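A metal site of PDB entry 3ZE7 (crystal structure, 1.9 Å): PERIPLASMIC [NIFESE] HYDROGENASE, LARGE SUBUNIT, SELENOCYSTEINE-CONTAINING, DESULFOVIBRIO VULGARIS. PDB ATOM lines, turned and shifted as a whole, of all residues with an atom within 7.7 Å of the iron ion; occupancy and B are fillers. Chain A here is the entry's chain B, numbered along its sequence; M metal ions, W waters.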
ATOM      1  N   GLU A  45     -20.070 -24.440  22.735  1.00  0.00           N
ATOM      2  CA  GLU A  45     -20.995 -25.265  21.991  1.00  0.00           C
ATOM      3  C   GLU A  45     -21.157 -26.653  22.602  1.00  0.00           C
ATOM      4  O   GLU A  45     -22.218 -27.235  22.522  1.00  0.00           O
ATOM      5  CB  GLU A  45     -20.594 -25.306  20.515  1.00  0.00           C
ATOM      6  CG  GLU A  45     -20.813 -23.944  19.841  1.00  0.00           C
ATOM      7  CD  GLU A  45     -19.990 -23.761  18.586  1.00  0.00           C
ATOM      8  OE1 GLU A  45     -18.922 -24.408  18.487  1.00  0.00           O
ATOM      9  OE2 GLU A  45     -20.403 -22.950  17.705  1.00  0.00           O
ATOM     10  N   GLU A 271     -19.078 -24.076   7.396  1.00  0.00           N
ATOM     11  CA  GLU A 271     -17.864 -23.868   8.165  1.00  0.00           C
ATOM     12  C   GLU A 271     -16.816 -24.937   7.867  1.00  0.00           C
ATOM     13  O   GLU A 271     -17.052 -26.125   8.088  1.00  0.00           O
ATOM     14  CB  GLU A 271     -18.169 -23.806   9.668  1.00  0.00           C
ATOM     15  CG  GLU A 271     -18.932 -22.555  10.076  1.00  0.00           C
ATOM     16  CD  GLU A 271     -19.077 -22.436  11.589  1.00  0.00           C
ATOM     17  OE1 GLU A 271     -19.922 -23.145  12.161  1.00  0.00           O
ATOM     18  OE2 GLU A 271     -18.341 -21.642  12.209  1.00  0.00           O
ATOM     19  N   PHE A 278      -9.840 -28.634  14.679  1.00  0.00           N
ATOM     20  CA  PHE A 278     -11.034 -29.434  14.876  1.00  0.00           C
ATOM     21  C   PHE A 278     -10.962 -30.677  14.002  1.00  0.00           C
ATOM     22  O   PHE A 278     -10.283 -30.692  12.977  1.00  0.00           O
ATOM     23  CB  PHE A 278     -12.291 -28.625  14.561  1.00  0.00           C
ATOM     24  CG  PHE A 278     -12.466 -27.426  15.436  1.00  0.00           C
ATOM     25  CD1 PHE A 278     -13.020 -27.553  16.700  1.00  0.00           C
ATOM     26  CD2 PHE A 278     -12.043 -26.169  15.000  1.00  0.00           C
ATOM     27  CE1 PHE A 278     -13.164 -26.456  17.517  1.00  0.00           C
ATOM     28  CE2 PHE A 278     -12.186 -25.057  15.820  1.00  0.00           C
ATOM     29  CZ  PHE A 278     -12.750 -25.199  17.085  1.00  0.00           C
ATOM     30  N   TYR A 287     -24.413 -24.533   9.950  1.00  0.00           N
ATOM     31  CA  TYR A 287     -24.580 -24.427  11.405  1.00  0.00           C
ATOM     32  C   TYR A 287     -25.680 -25.344  11.959  1.00  0.00           C
ATOM     33  O   TYR A 287     -25.593 -25.816  13.096  1.00  0.00           O
ATOM     34  CB  TYR A 287     -24.823 -22.971  11.816  1.00  0.00           C
ATOM     35  CG  TYR A 287     -26.043 -22.353  11.167  1.00  0.00           C
ATOM     36  CD1 TYR A 287     -27.307 -22.533  11.716  1.00  0.00           C
ATOM     37  CD2 TYR A 287     -25.921 -21.602  10.008  1.00  0.00           C
ATOM     38  CE1 TYR A 287     -28.433 -21.974  11.119  1.00  0.00           C
ATOM     39  CE2 TYR A 287     -27.055 -21.031   9.395  1.00  0.00           C
ATOM     40  CZ  TYR A 287     -28.293 -21.221   9.953  1.00  0.00           C
ATOM     41  OH  TYR A 287     -29.416 -20.671   9.361  1.00  0.00           O
ATOM     42  N   LYS A 291     -20.879 -29.135  14.280  1.00  0.00           N
ATOM     43  CA  LYS A 291     -20.239 -30.033  15.212  1.00  0.00           C
ATOM     44  C   LYS A 291     -18.965 -29.377  15.673  1.00  0.00           C
ATOM     45  O   LYS A 291     -18.290 -28.703  14.887  1.00  0.00           O
ATOM     46  CB  LYS A 291     -19.901 -31.343  14.520  1.00  0.00           C
ATOM     47  CG  LYS A 291     -21.030 -32.359  14.522  1.00  0.00           C
ATOM     48  CD  LYS A 291     -20.623 -33.595  13.726  1.00  0.00           C
ATOM     49  CE  LYS A 291     -21.308 -34.839  14.242  1.00  0.00           C
ATOM     50  NZ  LYS A 291     -22.785 -34.658  14.324  1.00  0.00           N
ATOM     51  N   THR A 292     -18.618 -29.570  16.943  1.00  0.00           N
ATOM     52  CA  THR A 292     -17.453 -28.921  17.531  1.00  0.00           C
ATOM     53  C   THR A 292     -16.603 -29.963  18.272  1.00  0.00           C
ATOM     54  O   THR A 292     -16.791 -30.229  19.462  1.00  0.00           O
ATOM     55  CB  THR A 292     -17.870 -27.734  18.422  1.00  0.00           C
ATOM     56  OG1 THR A 292     -18.611 -26.802  17.626  1.00  0.00           O
ATOM     57  CG2 THR A 292     -16.645 -27.001  19.024  1.00  0.00           C
ATOM     58  N   PHE A 304      -7.917 -21.841  16.317  1.00  0.00           N
ATOM     59  CA  PHE A 304      -9.159 -22.356  16.904  1.00  0.00           C
ATOM     60  C   PHE A 304     -10.416 -21.729  16.273  1.00  0.00           C
ATOM     61  O   PHE A 304     -11.546 -22.039  16.661  1.00  0.00           O
ATOM     62  CB  PHE A 304      -9.171 -22.157  18.421  1.00  0.00           C
ATOM     63  CG  PHE A 304      -8.284 -23.113  19.170  1.00  0.00           C
ATOM     64  CD1 PHE A 304      -8.518 -24.491  19.128  1.00  0.00           C
ATOM     65  CD2 PHE A 304      -7.230 -22.641  19.940  1.00  0.00           C
ATOM     66  CE1 PHE A 304      -7.720 -25.378  19.840  1.00  0.00           C
ATOM     67  CE2 PHE A 304      -6.426 -23.531  20.665  1.00  0.00           C
ATOM     68  CZ  PHE A 304      -6.669 -24.897  20.607  1.00  0.00           C
ATOM     69  N   LYS A 306     -12.934 -21.504  13.241  1.00  0.00           N
ATOM     70  CA  LYS A 306     -13.398 -22.185  12.045  1.00  0.00           C
ATOM     71  C   LYS A 306     -13.400 -21.207  10.862  1.00  0.00           C
ATOM     72  O   LYS A 306     -13.214 -20.004  11.051  1.00  0.00           O
ATOM     73  CB  LYS A 306     -14.813 -22.766  12.243  1.00  0.00           C
ATOM     74  CG  LYS A 306     -14.926 -23.929  13.224  1.00  0.00           C
ATOM     75  CD  LYS A 306     -16.362 -24.455  13.335  1.00  0.00           C
ATOM     76  CE  LYS A 306     -16.489 -25.596  14.368  1.00  0.00           C
ATOM     77  NZ  LYS A 306     -17.926 -25.905  14.725  1.00  0.00           N
ATOM     78  N   LEU A 415     -25.104 -15.258  14.550  1.00  0.00           N
ATOM     79  CA  LEU A 415     -26.253 -16.135  14.705  1.00  0.00           C
ATOM     80  C   LEU A 415     -26.007 -17.243  15.726  1.00  0.00           C
ATOM     81  O   LEU A 415     -24.866 -17.686  15.917  1.00  0.00           O
ATOM     82  CB  LEU A 415     -26.731 -16.717  13.368  1.00  0.00           C
ATOM     83  CG  LEU A 415     -25.931 -17.810  12.669  1.00  0.00           C
ATOM     84  CD1 LEU A 415     -26.362 -19.213  13.123  1.00  0.00           C
ATOM     85  CD2 LEU A 415     -26.044 -17.673  11.160  1.00  0.00           C
ATOM     86  N   TYR A 428     -26.071 -26.772  19.989  1.00  0.00           N
ATOM     87  CA  TYR A 428     -26.064 -25.319  20.001  1.00  0.00           C
ATOM     88  C   TYR A 428     -24.871 -24.901  19.160  1.00  0.00           C
ATOM     89  O   TYR A 428     -23.753 -25.310  19.436  1.00  0.00           O
ATOM     90  CB  TYR A 428     -25.957 -24.765  21.431  1.00  0.00           C
ATOM     91  CG  TYR A 428     -26.470 -23.342  21.625  1.00  0.00           C
ATOM     92  CD1 TYR A 428     -25.772 -22.222  21.131  1.00  0.00           C
ATOM     93  CD2 TYR A 428     -27.658 -23.109  22.322  1.00  0.00           C
ATOM     94  CE1 TYR A 428     -26.256 -20.913  21.336  1.00  0.00           C
ATOM     95  CE2 TYR A 428     -28.142 -21.814  22.522  1.00  0.00           C
ATOM     96  CZ  TYR A 428     -27.450 -20.730  22.029  1.00  0.00           C
ATOM     97  OH  TYR A 428     -27.947 -19.454  22.246  1.00  0.00           O
ATOM     98  N   GLN A 429     -25.112 -24.122  18.106  1.00  0.00           N
ATOM     99  CA  GLN A 429     -24.046 -23.712  17.216  1.00  0.00           C
ATOM    100  C   GLN A 429     -24.028 -22.197  17.088  1.00  0.00           C
ATOM    101  O   GLN A 429     -25.074 -21.561  16.918  1.00  0.00           O
ATOM    102  CB  GLN A 429     -24.199 -24.388  15.851  1.00  0.00           C
ATOM    103  CG  GLN A 429     -23.806 -25.867  15.855  1.00  0.00           C
ATOM    104  CD  GLN A 429     -22.314 -26.067  16.096  1.00  0.00           C
ATOM    105  OE1 GLN A 429     -21.483 -25.369  15.511  1.00  0.00           O
ATOM    106  NE2 GLN A 429     -21.971 -27.031  16.947  1.00  0.00           N
ATOM    107  N   ILE A 430     -22.822 -21.624  17.197  1.00  0.00           N
ATOM    108  CA  ILE A 430     -22.627 -20.180  17.163  1.00  0.00           C
ATOM    109  C   ILE A 430     -21.762 -19.805  15.984  1.00  0.00           C
ATOM    110  O   ILE A 430     -20.692 -20.364  15.781  1.00  0.00           O
ATOM    111  CB  ILE A 430     -21.976 -19.644  18.482  1.00  0.00           C
ATOM    112  CG1 ILE A 430     -22.923 -19.872  19.660  1.00  0.00           C
ATOM    113  CG2 ILE A 430     -21.610 -18.163  18.343  1.00  0.00           C
ATOM    114  CD1 ILE A 430     -22.257 -20.264  20.908  1.00  0.00           C
ATOM    115  N   VAL A 431     -22.253 -18.859  15.192  1.00  0.00           N
ATOM    116  CA  VAL A 431     -21.492 -18.324  14.072  1.00  0.00           C
ATOM    117  C   VAL A 431     -21.404 -16.821  14.294  1.00  0.00           C
ATOM    118  O   VAL A 431     -22.385 -16.111  14.069  1.00  0.00           O
ATOM    119  CB  VAL A 431     -22.179 -18.653  12.724  1.00  0.00           C
ATOM    120  CG1 VAL A 431     -21.445 -17.992  11.548  1.00  0.00           C
ATOM    121  CG2 VAL A 431     -22.246 -20.176  12.519  1.00  0.00           C
ATOM    122  N   SER A 432     -20.246 -16.364  14.759  1.00  0.00           N
ATOM    123  CA  SER A 432     -20.090 -15.009  15.292  1.00  0.00           C
ATOM    124  C   SER A 432     -19.392 -14.028  14.360  1.00  0.00           C
ATOM    125  O   SER A 432     -18.877 -14.403  13.305  1.00  0.00           O
ATOM    126  CB  SER A 432     -19.315 -15.076  16.608  1.00  0.00           C
ATOM    127  OG  SER A 432     -18.035 -15.636  16.361  1.00  0.00           O
ATOM    128  N   LEU A 435     -15.574 -14.390  13.891  1.00  0.00           N
ATOM    129  CA  LEU A 435     -15.439 -15.619  13.121  1.00  0.00           C
ATOM    130  C   LEU A 435     -15.409 -15.292  11.618  1.00  0.00           C
ATOM    131  O   LEU A 435     -14.556 -15.785  10.876  1.00  0.00           O
ATOM    132  CB  LEU A 435     -16.618 -16.546  13.427  1.00  0.00           C
ATOM    133  CG  LEU A 435     -16.831 -17.740  12.509  1.00  0.00           C
ATOM    134  CD1 LEU A 435     -15.696 -18.771  12.647  1.00  0.00           C
ATOM    135  CD2 LEU A 435     -18.181 -18.369  12.800  1.00  0.00           C
ATOM    136  N   CYS A 481     -15.058 -14.110  20.912  1.00  0.00           N
ATOM    137  CA  CYS A 481     -16.193 -14.360  20.033  1.00  0.00           C
ATOM    138  C   CYS A 481     -15.869 -15.274  18.861  1.00  0.00           C
ATOM    139  O   CYS A 481     -16.673 -16.131  18.509  1.00  0.00           O
ATOM    140  CB  CYS A 481     -16.752 -13.039  19.475  1.00  0.00           C
ATOM    141  SG  CYS A 481     -17.895 -12.251  20.574  1.00  0.00           S
ATOM    142  N   ALA A 482     -14.705 -15.099  18.251  1.00  0.00           N
ATOM    143  CA  ALA A 482     -14.381 -15.857  17.044  1.00  0.00           C
ATOM    144  C   ALA A 482     -14.315 -17.371  17.326  1.00  0.00           C
ATOM    145  O   ALA A 482     -14.739 -18.189  16.506  1.00  0.00           O
ATOM    146  CB  ALA A 482     -13.059 -15.364  16.407  1.00  0.00           C
ATOM    147  N   VAL A 483     -13.787 -17.724  18.486  1.00  0.00           N
ATOM    148  CA  VAL A 483     -13.572 -19.128  18.846  1.00  0.00           C
ATOM    149  C   VAL A 483     -14.678 -19.697  19.725  1.00  0.00           C
ATOM    150  O   VAL A 483     -15.121 -20.835  19.509  1.00  0.00           O
ATOM    151  CB  VAL A 483     -12.243 -19.298  19.599  1.00  0.00           C
ATOM    152  CG1 VAL A 483     -12.047 -20.759  19.975  1.00  0.00           C
ATOM    153  CG2 VAL A 483     -11.059 -18.759  18.772  1.00  0.00           C
ATOM    154  N   HIS A 484     -15.140 -18.899  20.685  1.00  0.00           N
ATOM    155  CA  HIS A 484     -16.060 -19.373  21.725  1.00  0.00           C
ATOM    156  C   HIS A 484     -15.765 -20.815  22.190  1.00  0.00           C
ATOM    157  O   HIS A 484     -14.595 -21.113  22.465  1.00  0.00           O
ATOM    158  CB  HIS A 484     -17.531 -19.206  21.313  1.00  0.00           C
ATOM    159  CG  HIS A 484     -17.806 -19.601  19.891  1.00  0.00           C
ATOM    160  ND1 HIS A 484     -17.533 -18.776  18.831  1.00  0.00           N
ATOM    161  CD2 HIS A 484     -18.322 -20.731  19.366  1.00  0.00           C
ATOM    162  CE1 HIS A 484     -17.859 -19.380  17.700  1.00  0.00           C
ATOM    163  NE2 HIS A 484     -18.346 -20.576  17.998  1.00  0.00           N
ATOM    164  OXT HIS A 484     -16.633 -21.689  22.285  1.00  0.00           O
HETATM  165 FE    FE M   1     -19.072 -21.885  16.300  1.00  0.00          FE
HETATM  166  O   HOH W   1     -19.947 -23.211  14.735  1.00  0.00           O
HETATM  167  O   HOH W   2     -17.264 -23.414  16.637  1.00  0.00           O
HETATM  168  O   HOH W   3     -17.668 -20.993  14.597  1.00  0.00           O
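Of the 19 residues printed, 3 come within 4 Å of the iron ion. The nearest printed residue that does not touch the iron ion is Glu 271 (4.2 Å).
The iron ion is bound by the side-chain carboxylate (OE2) of Glu 45 (2.2 Å), water W1 (2.2 Å), a ring nitrogen (NE2) of His 484 (2.3 Å), the backbone carbonyl oxygen (O) of Ile 430 (2.3 Å), water W3 (2.4 Å) and water W2 (2.4 Å). The iron ion has six donor atoms within binding distance.
Water W2 bridges the side-chain carboxylate of Glu 45 (2.7 Å) and the side-chain amino group of Lys 306 (3.2 Å). Water W1 lies within hydrogen-bond range of the side-chain carboxylate (OE1) of Glu 271 (2.6 Å), the side-chain amide oxygen (OE1) of Gln 429 (2.8 Å) and the side-chain amino group (NZ) of Lys 306 (3.4 Å).
A ring nitrogen (ND1) of His 484 is in hydrogen-bond range of the backbone carbonyl oxygen (O) of Cys 481, at 2.8 Å. OE1 of Gln 429 sits close to OE2 of Glu 45, 3.4 Å away. The side-chain carboxylate (OE1) of Glu 45 is in hydrogen-bond range of the side-chain hydroxyl (OG1) of Thr 292 (2.6 Å).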
